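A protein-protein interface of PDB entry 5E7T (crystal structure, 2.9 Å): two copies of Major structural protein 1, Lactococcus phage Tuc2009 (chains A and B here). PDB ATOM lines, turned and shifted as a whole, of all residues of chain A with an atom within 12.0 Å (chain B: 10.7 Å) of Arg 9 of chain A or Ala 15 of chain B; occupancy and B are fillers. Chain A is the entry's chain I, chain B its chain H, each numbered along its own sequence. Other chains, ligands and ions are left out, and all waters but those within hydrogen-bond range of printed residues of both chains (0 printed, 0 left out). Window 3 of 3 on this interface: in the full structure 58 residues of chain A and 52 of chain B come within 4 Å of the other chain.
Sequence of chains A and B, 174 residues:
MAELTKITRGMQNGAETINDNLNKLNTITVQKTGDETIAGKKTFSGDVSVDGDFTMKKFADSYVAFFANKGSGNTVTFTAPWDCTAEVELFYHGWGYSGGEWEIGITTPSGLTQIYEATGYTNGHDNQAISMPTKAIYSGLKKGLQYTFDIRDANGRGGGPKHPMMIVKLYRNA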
ATOM      1  N   LEU A   4     -34.458  11.661  31.176  1.00  0.00           N
ATOM      2  CA  LEU A   4     -33.090  11.962  30.756  1.00  0.00           C
ATOM      3  C   LEU A   4     -32.974  13.458  30.506  1.00  0.00           C
ATOM      4  O   LEU A   4     -33.925  14.070  30.017  1.00  0.00           O
ATOM      5  CB  LEU A   4     -32.706  11.214  29.478  1.00  0.00           C
ATOM      6  CG  LEU A   4     -32.751   9.702  29.484  1.00  0.00           C
ATOM      7  CD1 LEU A   4     -32.389   9.178  28.143  1.00  0.00           C
ATOM      8  CD2 LEU A   4     -31.834   9.113  30.532  1.00  0.00           C
ATOM      9  N   THR A   5     -31.815  14.046  30.816  1.00  0.00           N
ATOM     10  CA  THR A   5     -31.610  15.481  30.607  1.00  0.00           C
ATOM     11  C   THR A   5     -31.104  15.683  29.175  1.00  0.00           C
ATOM     12  O   THR A   5     -30.155  15.036  28.754  1.00  0.00           O
ATOM     13  CB  THR A   5     -30.804  16.174  31.746  1.00  0.00           C
ATOM     14  OG1 THR A   5     -29.989  17.226  31.211  1.00  0.00           O
ATOM     15  CG2 THR A   5     -29.999  15.207  32.620  1.00  0.00           C
ATOM     16  N   LYS A   6     -31.801  16.553  28.419  1.00  0.00           N
ATOM     17  CA  LYS A   6     -31.550  16.830  27.006  1.00  0.00           C
ATOM     18  C   LYS A   6     -30.120  17.219  26.719  1.00  0.00           C
ATOM     19  O   LYS A   6     -29.575  18.061  27.427  1.00  0.00           O
ATOM     20  CB  LYS A   6     -32.539  17.892  26.478  1.00  0.00           C
ATOM     21  CG  LYS A   6     -32.679  17.911  24.958  1.00  0.00           C
ATOM     22  CD  LYS A   6     -33.546  19.071  24.489  1.00  0.00           C
ATOM     23  CE  LYS A   6     -33.528  19.260  22.990  1.00  0.00           C
ATOM     24  NZ  LYS A   6     -34.860  19.608  22.440  1.00  0.00           N
ATOM     25  N   ILE A   7     -29.529  16.598  25.679  1.00  0.00           N
ATOM     26  CA  ILE A   7     -28.186  16.863  25.151  1.00  0.00           C
ATOM     27  C   ILE A   7     -28.368  17.819  23.964  1.00  0.00           C
ATOM     28  O   ILE A   7     -28.981  17.446  22.951  1.00  0.00           O
ATOM     29  CB  ILE A   7     -27.462  15.547  24.741  1.00  0.00           C
ATOM     30  CG1 ILE A   7     -27.361  14.542  25.908  1.00  0.00           C
ATOM     31  CG2 ILE A   7     -26.104  15.813  24.104  1.00  0.00           C
ATOM     32  CD1 ILE A   7     -26.785  15.059  27.165  1.00  0.00           C
ATOM     33  N   THR A   8     -27.891  19.063  24.121  1.00  0.00           N
ATOM     34  CA  THR A   8     -28.035  20.103  23.112  1.00  0.00           C
ATOM     35  C   THR A   8     -26.684  20.660  22.649  1.00  0.00           C
ATOM     36  O   THR A   8     -25.708  20.623  23.397  1.00  0.00           O
ATOM     37  CB  THR A   8     -28.930  21.256  23.651  1.00  0.00           C
ATOM     38  OG1 THR A   8     -28.321  21.875  24.786  1.00  0.00           O
ATOM     39  CG2 THR A   8     -30.320  20.816  23.999  1.00  0.00           C
ATOM     40  N   ARG A   9     -26.654  21.225  21.429  1.00  0.00           N
ATOM     41  CA  ARG A   9     -25.510  21.917  20.861  1.00  0.00           C
ATOM     42  C   ARG A   9     -25.184  23.108  21.747  1.00  0.00           C
ATOM     43  O   ARG A   9     -26.086  23.896  22.093  1.00  0.00           O
ATOM     44  CB  ARG A   9     -25.863  22.417  19.451  1.00  0.00           C
ATOM     45  CG  ARG A   9     -24.781  23.241  18.743  1.00  0.00           C
ATOM     46  CD  ARG A   9     -25.153  23.485  17.295  1.00  0.00           C
ATOM     47  NE  ARG A   9     -26.280  24.410  17.187  1.00  0.00           N
ATOM     48  CZ  ARG A   9     -26.153  25.706  16.937  1.00  0.00           C
ATOM     49  NH1 ARG A   9     -24.946  26.242  16.749  1.00  0.00           N
ATOM     50  NH2 ARG A   9     -27.229  26.479  16.860  1.00  0.00           N
ATOM     51  N   GLY A  10     -23.917  23.196  22.130  1.00  0.00           N
ATOM     52  CA  GLY A  10     -23.374  24.295  22.911  1.00  0.00           C
ATOM     53  C   GLY A  10     -23.621  24.254  24.401  1.00  0.00           C
ATOM     54  O   GLY A  10     -23.222  25.186  25.121  1.00  0.00           O
ATOM     55  N   MET A  11     -24.250  23.161  24.888  1.00  0.00           N
ATOM     56  CA  MET A  11     -24.524  23.002  26.314  1.00  0.00           C
ATOM     57  C   MET A  11     -23.212  23.017  27.098  1.00  0.00           C
ATOM     58  O   MET A  11     -22.180  22.577  26.580  1.00  0.00           O
ATOM     59  CB  MET A  11     -25.384  21.755  26.591  1.00  0.00           C
ATOM     60  CG  MET A  11     -24.620  20.452  26.566  1.00  0.00           C
ATOM     61  SD  MET A  11     -25.635  18.985  26.859  1.00  0.00           S
ATOM     62  CE  MET A  11     -26.257  19.299  28.435  1.00  0.00           C
ATOM     63  N   GLN A  12     -23.239  23.583  28.311  1.00  0.00           N
ATOM     64  CA  GLN A  12     -22.070  23.728  29.159  1.00  0.00           C
ATOM     65  C   GLN A  12     -21.487  22.402  29.659  1.00  0.00           C
ATOM     66  O   GLN A  12     -20.282  22.254  29.514  1.00  0.00           O
ATOM     67  CB  GLN A  12     -22.375  24.690  30.303  1.00  0.00           C
ATOM     68  CG  GLN A  12     -21.354  24.772  31.419  1.00  0.00           C
ATOM     69  CD  GLN A  12     -21.505  26.038  32.202  1.00  0.00           C
ATOM     70  OE1 GLN A  12     -21.721  27.106  31.647  1.00  0.00           O
ATOM     71  NE2 GLN A  12     -21.361  25.966  33.513  1.00  0.00           N
ATOM     72  N   ASN A  13     -22.276  21.465  30.262  1.00  0.00           N
ATOM     73  CA  ASN A  13     -21.719  20.206  30.795  1.00  0.00           C
ATOM     74  C   ASN A  13     -22.171  18.984  29.999  1.00  0.00           C
ATOM     75  O   ASN A  13     -22.815  18.065  30.520  1.00  0.00           O
ATOM     76  CB  ASN A  13     -21.986  20.062  32.286  1.00  0.00           C
ATOM     77  CG  ASN A  13     -21.405  21.202  33.093  1.00  0.00           C
ATOM     78  OD1 ASN A  13     -20.203  21.493  33.039  1.00  0.00           O
ATOM     79  ND2 ASN A  13     -22.250  21.886  33.855  1.00  0.00           N
ATOM     80  N   GLY A  14     -21.804  19.010  28.720  1.00  0.00           N
ATOM     81  CA  GLY A  14     -22.123  17.987  27.732  1.00  0.00           C
ATOM     82  C   GLY A  14     -21.596  16.622  28.085  1.00  0.00           C
ATOM     83  O   GLY A  14     -22.365  15.671  28.127  1.00  0.00           O
ATOM     84  N   ALA A  15     -20.304  16.527  28.398  1.00  0.00           N
ATOM     85  CA  ALA A  15     -19.644  15.291  28.781  1.00  0.00           C
ATOM     86  C   ALA A  15     -20.289  14.680  30.009  1.00  0.00           C
ATOM     87  O   ALA A  15     -20.616  13.485  29.997  1.00  0.00           O
ATOM     88  CB  ALA A  15     -18.168  15.554  29.043  1.00  0.00           C
ATOM     89  N   GLU A  16     -20.518  15.528  31.046  1.00  0.00           N
ATOM     90  CA  GLU A  16     -21.107  15.160  32.344  1.00  0.00           C
ATOM     91  C   GLU A  16     -22.554  14.713  32.214  1.00  0.00           C
ATOM     92  O   GLU A  16     -22.949  13.767  32.899  1.00  0.00           O
ATOM     93  CB  GLU A  16     -21.005  16.319  33.335  1.00  0.00           C
ATOM     94  CG  GLU A  16     -19.587  16.685  33.701  1.00  0.00           C
ATOM     95  CD  GLU A  16     -18.891  17.690  32.812  1.00  0.00           C
ATOM     96  OE1 GLU A  16     -19.454  18.039  31.751  1.00  0.00           O
ATOM     97  OE2 GLU A  16     -17.737  18.055  33.133  1.00  0.00           O
ATOM     98  N   THR A  17     -23.338  15.379  31.343  1.00  0.00           N
ATOM     99  CA  THR A  17     -24.739  15.037  31.144  1.00  0.00           C
ATOM    100  C   THR A  17     -24.865  13.752  30.327  1.00  0.00           C
ATOM    101  O   THR A  17     -25.737  12.934  30.642  1.00  0.00           O
ATOM    102  CB  THR A  17     -25.535  16.220  30.597  1.00  0.00           C
ATOM    103  OG1 THR A  17     -25.301  17.388  31.399  1.00  0.00           O
ATOM    104  CG2 THR A  17     -27.002  15.949  30.571  1.00  0.00           C
ATOM    105  N   ILE A  18     -23.975  13.542  29.321  1.00  0.00           N
ATOM    106  CA  ILE A  18     -23.957  12.311  28.518  1.00  0.00           C
ATOM    107  C   ILE A  18     -23.665  11.147  29.452  1.00  0.00           C
ATOM    108  O   ILE A  18     -24.397  10.152  29.426  1.00  0.00           O
ATOM    109  CB  ILE A  18     -22.952  12.379  27.319  1.00  0.00           C
ATOM    110  CG1 ILE A  18     -23.443  13.380  26.246  1.00  0.00           C
ATOM    111  CG2 ILE A  18     -22.691  10.991  26.699  1.00  0.00           C
ATOM    112  CD1 ILE A  18     -22.406  13.870  25.268  1.00  0.00           C
ATOM    113  N   ASN A  19     -22.628  11.283  30.309  1.00  0.00           N
ATOM    114  CA  ASN A  19     -22.266  10.224  31.248  1.00  0.00           C
ATOM    115  C   ASN A  19     -23.462   9.893  32.105  1.00  0.00           C
ATOM    116  O   ASN A  19     -23.881   8.742  32.138  1.00  0.00           O
ATOM    117  CB  ASN A  19     -21.078  10.621  32.104  1.00  0.00           C
ATOM    118  CG  ASN A  19     -20.457   9.470  32.839  1.00  0.00           C
ATOM    119  OD1 ASN A  19     -20.124   8.435  32.256  1.00  0.00           O
ATOM    120  ND2 ASN A  19     -20.287   9.624  34.144  1.00  0.00           N
ATOM    121  N   ASN A  21     -26.765  10.383  31.646  1.00  0.00           N
ATOM    122  CA  ASN A  21     -27.853   9.738  30.908  1.00  0.00           C
ATOM    123  C   ASN A  21     -27.533   8.286  30.605  1.00  0.00           C
ATOM    124  O   ASN A  21     -28.414   7.443  30.762  1.00  0.00           O
ATOM    125  CB  ASN A  21     -28.175  10.499  29.647  1.00  0.00           C
ATOM    126  CG  ASN A  21     -28.800  11.846  29.901  1.00  0.00           C
ATOM    127  OD1 ASN A  21     -29.377  12.133  30.968  1.00  0.00           O
ATOM    128  ND2 ASN A  21     -28.729  12.685  28.890  1.00  0.00           N
ATOM    129  N   LEU A  22     -26.262   7.979  30.250  1.00  0.00           N
ATOM    130  CA  LEU A  22     -25.803   6.616  30.003  1.00  0.00           C
ATOM    131  C   LEU A  22     -25.892   5.803  31.289  1.00  0.00           C
ATOM    132  O   LEU A  22     -26.371   4.672  31.258  1.00  0.00           O
ATOM    133  CB  LEU A  22     -24.368   6.604  29.468  1.00  0.00           C
ATOM    134  CG  LEU A  22     -24.142   7.128  28.058  1.00  0.00           C
ATOM    135  CD1 LEU A  22     -22.672   7.336  27.812  1.00  0.00           C
ATOM    136  CD2 LEU A  22     -24.744   6.214  27.011  1.00  0.00           C
ATOM    137  N   THR B   5     -27.908   5.587  15.323  1.00  0.00           N
ATOM    138  CA  THR B   5     -27.036   6.196  14.326  1.00  0.00           C
ATOM    139  C   THR B   5     -25.635   6.383  14.959  1.00  0.00           C
ATOM    140  O   THR B   5     -25.511   6.936  16.050  1.00  0.00           O
ATOM    141  CB  THR B   5     -27.661   7.445  13.636  1.00  0.00           C
ATOM    142  OG1 THR B   5     -26.653   8.428  13.369  1.00  0.00           O
ATOM    143  CG2 THR B   5     -28.854   8.042  14.393  1.00  0.00           C
ATOM    144  N   LYS B   6     -24.595   5.871  14.277  1.00  0.00           N
ATOM    145  CA  LYS B   6     -23.191   5.886  14.712  1.00  0.00           C
ATOM    146  C   LYS B   6     -22.688   7.269  15.033  1.00  0.00           C
ATOM    147  O   LYS B   6     -22.916   8.204  14.258  1.00  0.00           O
ATOM    148  CB  LYS B   6     -22.292   5.239  13.649  1.00  0.00           C
ATOM    149  CG  LYS B   6     -20.907   4.832  14.120  1.00  0.00           C
ATOM    150  CD  LYS B   6     -20.047   4.365  12.960  1.00  0.00           C
ATOM    151  CE  LYS B   6     -18.655   3.999  13.388  1.00  0.00           C
ATOM    152  NZ  LYS B   6     -17.940   3.221  12.338  1.00  0.00           N
ATOM    153  N   ILE B   7     -21.998   7.377  16.192  1.00  0.00           N
ATOM    154  CA  ILE B   7     -21.370   8.584  16.730  1.00  0.00           C
ATOM    155  C   ILE B   7     -19.896   8.509  16.372  1.00  0.00           C
ATOM    156  O   ILE B   7     -19.177   7.639  16.862  1.00  0.00           O
ATOM    157  CB  ILE B   7     -21.607   8.743  18.259  1.00  0.00           C
ATOM    158  CG1 ILE B   7     -23.124   8.752  18.630  1.00  0.00           C
ATOM    159  CG2 ILE B   7     -20.870   9.949  18.846  1.00  0.00           C
ATOM    160  CD1 ILE B   7     -23.983   9.715  17.938  1.00  0.00           C
ATOM    161  N   THR B   8     -19.456   9.396  15.480  1.00  0.00           N
ATOM    162  CA  THR B   8     -18.079   9.452  15.014  1.00  0.00           C
ATOM    163  C   THR B   8     -17.461  10.820  15.261  1.00  0.00           C
ATOM    164  O   THR B   8     -18.188  11.807  15.256  1.00  0.00           O
ATOM    165  CB  THR B   8     -17.998   9.089  13.521  1.00  0.00           C
ATOM    166  OG1 THR B   8     -18.718  10.027  12.741  1.00  0.00           O
ATOM    167  CG2 THR B   8     -18.515   7.716  13.228  1.00  0.00           C
ATOM    168  N   ARG B   9     -16.124  10.894  15.450  1.00  0.00           N
ATOM    169  CA  ARG B   9     -15.417  12.171  15.588  1.00  0.00           C
ATOM    170  C   ARG B   9     -15.540  12.920  14.250  1.00  0.00           C
ATOM    171  O   ARG B   9     -15.383  12.317  13.192  1.00  0.00           O
ATOM    172  CB  ARG B   9     -13.944  11.911  15.872  1.00  0.00           C
ATOM    173  CG  ARG B   9     -13.079  13.166  16.086  1.00  0.00           C
ATOM    174  CD  ARG B   9     -11.658  12.837  16.555  1.00  0.00           C
ATOM    175  NE  ARG B   9     -11.608  11.567  17.287  1.00  0.00           N
ATOM    176  CZ  ARG B   9     -11.723  11.453  18.602  1.00  0.00           C
ATOM    177  NH1 ARG B   9     -11.789  12.533  19.366  1.00  0.00           N
ATOM    178  NH2 ARG B   9     -11.689  10.262  19.171  1.00  0.00           N
ATOM    179  N   GLY B  10     -15.868  14.195  14.309  1.00  0.00           N
ATOM    180  CA  GLY B  10     -16.024  15.029  13.126  1.00  0.00           C
ATOM    181  C   GLY B  10     -17.415  15.060  12.529  1.00  0.00           C
ATOM    182  O   GLY B  10     -17.655  15.820  11.587  1.00  0.00           O
ATOM    183  N   MET B  11     -18.341  14.243  13.054  1.00  0.00           N
ATOM    184  CA  MET B  11     -19.727  14.199  12.574  1.00  0.00           C
ATOM    185  C   MET B  11     -20.428  15.552  12.754  1.00  0.00           C
ATOM    186  O   MET B  11     -20.040  16.328  13.628  1.00  0.00           O
ATOM    187  CB  MET B  11     -20.516  13.046  13.224  1.00  0.00           C
ATOM    188  CG  MET B  11     -21.040  13.354  14.602  1.00  0.00           C
ATOM    189  SD  MET B  11     -21.935  11.991  15.301  1.00  0.00           S
ATOM    190  CE  MET B  11     -23.268  11.942  14.265  1.00  0.00           C
ATOM    191  N   GLN B  12     -21.491  15.796  11.972  1.00  0.00           N
ATOM    192  CA  GLN B  12     -22.173  17.074  11.926  1.00  0.00           C
ATOM    193  C   GLN B  12     -23.073  17.398  13.121  1.00  0.00           C
ATOM    194  O   GLN B  12     -22.875  18.468  13.745  1.00  0.00           O
ATOM    195  CB  GLN B  12     -22.931  17.251  10.625  1.00  0.00           C
ATOM    196  CG  GLN B  12     -22.000  17.569   9.462  1.00  0.00           C
ATOM    197  CD  GLN B  12     -22.578  18.606   8.539  1.00  0.00           C
ATOM    198  OE1 GLN B  12     -23.595  18.380   7.846  1.00  0.00           O
ATOM    199  NE2 GLN B  12     -21.938  19.775   8.529  1.00  0.00           N
ATOM    200  N   ASN B  13     -24.065  16.565  13.437  1.00  0.00           N
ATOM    201  CA  ASN B  13     -24.908  16.984  14.553  1.00  0.00           C
ATOM    202  C   ASN B  13     -24.728  16.037  15.705  1.00  0.00           C
ATOM    203  O   ASN B  13     -25.630  15.256  16.018  1.00  0.00           O
ATOM    204  CB  ASN B  13     -26.343  17.135  14.099  1.00  0.00           C
ATOM    205  CG  ASN B  13     -26.524  18.206  13.052  1.00  0.00           C
ATOM    206  OD1 ASN B  13     -26.168  19.373  13.262  1.00  0.00           O
ATOM    207  ND2 ASN B  13     -27.074  17.829  11.895  1.00  0.00           N
ATOM    208  N   GLY B  14     -23.531  16.082  16.282  1.00  0.00           N
ATOM    209  CA  GLY B  14     -23.091  15.194  17.342  1.00  0.00           C
ATOM    210  C   GLY B  14     -23.996  15.195  18.540  1.00  0.00           C
ATOM    211  O   GLY B  14     -24.491  14.140  18.927  1.00  0.00           O
ATOM    212  N   ALA B  15     -24.240  16.384  19.118  1.00  0.00           N
ATOM    213  CA  ALA B  15     -25.087  16.562  20.310  1.00  0.00           C
ATOM    214  C   ALA B  15     -26.514  16.052  20.068  1.00  0.00           C
ATOM    215  O   ALA B  15     -27.048  15.282  20.862  1.00  0.00           O
ATOM    216  CB  ALA B  15     -25.114  18.025  20.716  1.00  0.00           C
ATOM    217  N   GLU B  16     -27.084  16.437  18.939  1.00  0.00           N
ATOM    218  CA  GLU B  16     -28.426  16.091  18.499  1.00  0.00           C
ATOM    219  C   GLU B  16     -28.572  14.582  18.199  1.00  0.00           C
ATOM    220  O   GLU B  16     -29.625  14.031  18.496  1.00  0.00           O
ATOM    221  CB  GLU B  16     -28.812  16.944  17.273  1.00  0.00           C
ATOM    222  CG  GLU B  16     -28.786  18.456  17.488  1.00  0.00           C
ATOM    223  CD  GLU B  16     -27.502  19.207  17.177  1.00  0.00           C
ATOM    224  OE1 GLU B  16     -27.602  20.285  16.546  1.00  0.00           O
ATOM    225  OE2 GLU B  16     -26.407  18.754  17.586  1.00  0.00           O
ATOM    226  N   THR B  17     -27.533  13.917  17.613  1.00  0.00           N
ATOM    227  CA  THR B  17     -27.557  12.470  17.322  1.00  0.00           C
ATOM    228  C   THR B  17     -27.405  11.686  18.618  1.00  0.00           C
ATOM    229  O   THR B  17     -28.097  10.671  18.774  1.00  0.00           O
ATOM    230  CB  THR B  17     -26.534  12.073  16.254  1.00  0.00           C
ATOM    231  OG1 THR B  17     -26.711  12.924  15.114  1.00  0.00           O
ATOM    232  CG2 THR B  17     -26.654  10.607  15.834  1.00  0.00           C
ATOM    233  N   ILE B  18     -26.558  12.176  19.578  1.00  0.00           N
ATOM    234  CA  ILE B  18     -26.402  11.543  20.894  1.00  0.00           C
ATOM    235  C   ILE B  18     -27.758  11.631  21.615  1.00  0.00           C
ATOM    236  O   ILE B  18     -28.217  10.633  22.173  1.00  0.00           O
ATOM    237  CB  ILE B  18     -25.242  12.144  21.729  1.00  0.00           C
ATOM    238  CG1 ILE B  18     -23.874  11.851  21.072  1.00  0.00           C
ATOM    239  CG2 ILE B  18     -25.267  11.630  23.173  1.00  0.00           C
ATOM    240  CD1 ILE B  18     -22.759  12.719  21.517  1.00  0.00           C
ATOM    241  N   ASN B  19     -28.443  12.787  21.513  1.00  0.00           N
ATOM    242  CA  ASN B  19     -29.736  12.978  22.164  1.00  0.00           C
ATOM    243  C   ASN B  19     -30.771  12.035  21.629  1.00  0.00           C
ATOM    244  O   ASN B  19     -31.497  11.423  22.415  1.00  0.00           O
ATOM    245  CB  ASN B  19     -30.210  14.413  22.051  1.00  0.00           C
ATOM    246  CG  ASN B  19     -31.180  14.785  23.139  1.00  0.00           C
ATOM    247  OD1 ASN B  19     -30.890  14.664  24.340  1.00  0.00           O
ATOM    248  ND2 ASN B  19     -32.359  15.253  22.747  1.00  0.00           N
ATOM    249  N   ASP B  20     -30.803  11.869  20.294  1.00  0.00           N
ATOM    250  CA  ASP B  20     -31.762  10.986  19.640  1.00  0.00           C
ATOM    251  C   ASP B  20     -31.505   9.521  19.959  1.00  0.00           C
ATOM    252  O   ASP B  20     -32.472   8.766  20.110  1.00  0.00           O
ATOM    253  CB  ASP B  20     -31.811  11.239  18.134  1.00  0.00           C
ATOM    254  CG  ASP B  20     -32.399  12.573  17.734  1.00  0.00           C
ATOM    255  OD1 ASP B  20     -33.422  12.988  18.347  1.00  0.00           O
ATOM    256  OD2 ASP B  20     -31.887  13.176  16.767  1.00  0.00           O
ATOM    257  N   ASN B  21     -30.211   9.125  20.087  1.00  0.00           N
ATOM    258  CA  ASN B  21     -29.861   7.747  20.437  1.00  0.00           C
ATOM    259  C   ASN B  21     -30.264   7.441  21.879  1.00  0.00           C
ATOM    260  O   ASN B  21     -30.808   6.365  22.141  1.00  0.00           O
ATOM    261  CB  ASN B  21     -28.381   7.457  20.184  1.00  0.00           C
ATOM    262  CG  ASN B  21     -27.987   7.376  18.721  1.00  0.00           C
ATOM    263  OD1 ASN B  21     -28.801   7.168  17.816  1.00  0.00           O
ATOM    264  ND2 ASN B  21     -26.711   7.527  18.458  1.00  0.00           N
ATOM    265  N   LEU B  22     -30.060   8.415  22.797  1.00  0.00           N
ATOM    266  CA  LEU B  22     -30.432   8.275  24.203  1.00  0.00           C
ATOM    267  C   LEU B  22     -31.931   8.192  24.315  1.00  0.00           C
ATOM    268  O   LEU B  22     -32.437   7.347  25.051  1.00  0.00           O
ATOM    269  CB  LEU B  22     -29.892   9.422  25.062  1.00  0.00           C
ATOM    270  CG  LEU B  22     -28.373   9.456  25.287  1.00  0.00           C
ATOM    271  CD1 LEU B  22     -27.955  10.778  25.822  1.00  0.00           C
ATOM    272  CD2 LEU B  22     -27.916   8.350  26.214  1.00  0.00           C
ATOM    273  N   ASN B  23     -32.650   9.012  23.539  1.00  0.00           N
ATOM    274  CA  ASN B  23     -34.110   8.996  23.550  1.00  0.00           C
ATOM    275  C   ASN B  23     -34.678   7.680  22.988  1.00  0.00           C
ATOM    276  O   ASN B  23     -35.647   7.154  23.536  1.00  0.00           O
ATOM    277  CB  ASN B  23     -34.671  10.217  22.823  1.00  0.00           C
ATOM    278  CG  ASN B  23     -34.493  11.514  23.566  1.00  0.00           C
ATOM    279  OD1 ASN B  23     -34.304  11.557  24.791  1.00  0.00           O
ATOM    280  ND2 ASN B  23     -34.588  12.608  22.843  1.00  0.00           N
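OD1 of Asn 19 of chain B sits at hydrogen-bond distance from N of Ile 7 of chain A, 2.7 Å away.
O of Asn 19 of chain B lies close to ND2 of Asn 23 of chain B (3.3 Å).
ND2 of Asn 21 of chain A lies close to O of Thr 17 of chain A (3.5 Å).
The backbone carbonyl oxygen (O) of Thr 5 of chain A sits at hydrogen-bond distance from the side-chain amide nitrogen (ND2) of Asn 21 of chain A (2.8 Å).
The side-chain sulfur (SD) of Met 11 of chain A sits at hydrogen-bond distance from the backbone NH (N) of Thr 8 of chain A (3.5 Å).
Among the printed residues, merely in contact across the chains: Leu 4 of chain A with Leu 22 of chain B, Lys 6 of chain A with Asn 19 of chain B, Ile 7 of chain A with Ala 15 of chain B, Ile 7 of chain A with Leu 22 of chain B, Thr 8 of chain A with Ala 15 of chain B, Arg 9 of chain A with Ala 15 of chain B, Ile 18 of chain A with Ile 18 of chain B, Asn 21 of chain A with Leu 22 of chain B and Leu 22 of chain A with Leu 22 of chain B.
Of the printed residues of chain B, Arg 9 of chain A touches Ala 15.
Of chain A, only Ile 7 (3.4 Å), Thr 8 (3.6 Å) and Arg 9 (3.6 Å) come within 4 Å of Ala 15 of chain B.
No residue of chain A comes within 4 Å of Thr 17 of chain B.
Asn 19 of chain B touches just these residues of chain A: Lys 6 and Ile 7.
Of the printed residues of chain B, Leu 4 of chain A touches Leu 22.
Printed residues of chain B within 4 Å of Asn 21 of chain A: Leu 22 (3.7 Å).
Printed residues of chain B within 4 Å of Leu 22 of chain A: Leu 22 (3.9 Å).
The nearest residue of chain A that does not touch Ala 15 of chain B is Gly 10 of chain A (5.5 Å).
Hydrophobic or aromatic side chains of chain A within 4 Å of the printed part of chain B: Leu 4, Ile 7, Ile 18 and Leu 22.
Hydrophobic or aromatic side chains of chain B within 4 Å of the printed part of chain A: Ala 15, Ile 18 and Leu 22.
Ile 7 of chain A touches Asn 19 of chain B, but with the chains exchanged Asn 19 of chain A does not touch Ile 7 of chain B (11.7 Å).
Arg 9 of chain A touches Ala 15 of chain B, but with the chains exchanged Ala 15 of chain A does not touch Arg 9 of chain B (12.0 Å).
Ile 18 of chain A touches its own counterpart, Ile 18 of chain B.
Leu 22 of chain A touches its own counterpart, Leu 22 of chain B.
Positions printed for both chains: 5, 6, 7, 8, 9, 10, 11, 12, 13, 14, 15, 16, 17, 18, 19, 21 and 22.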
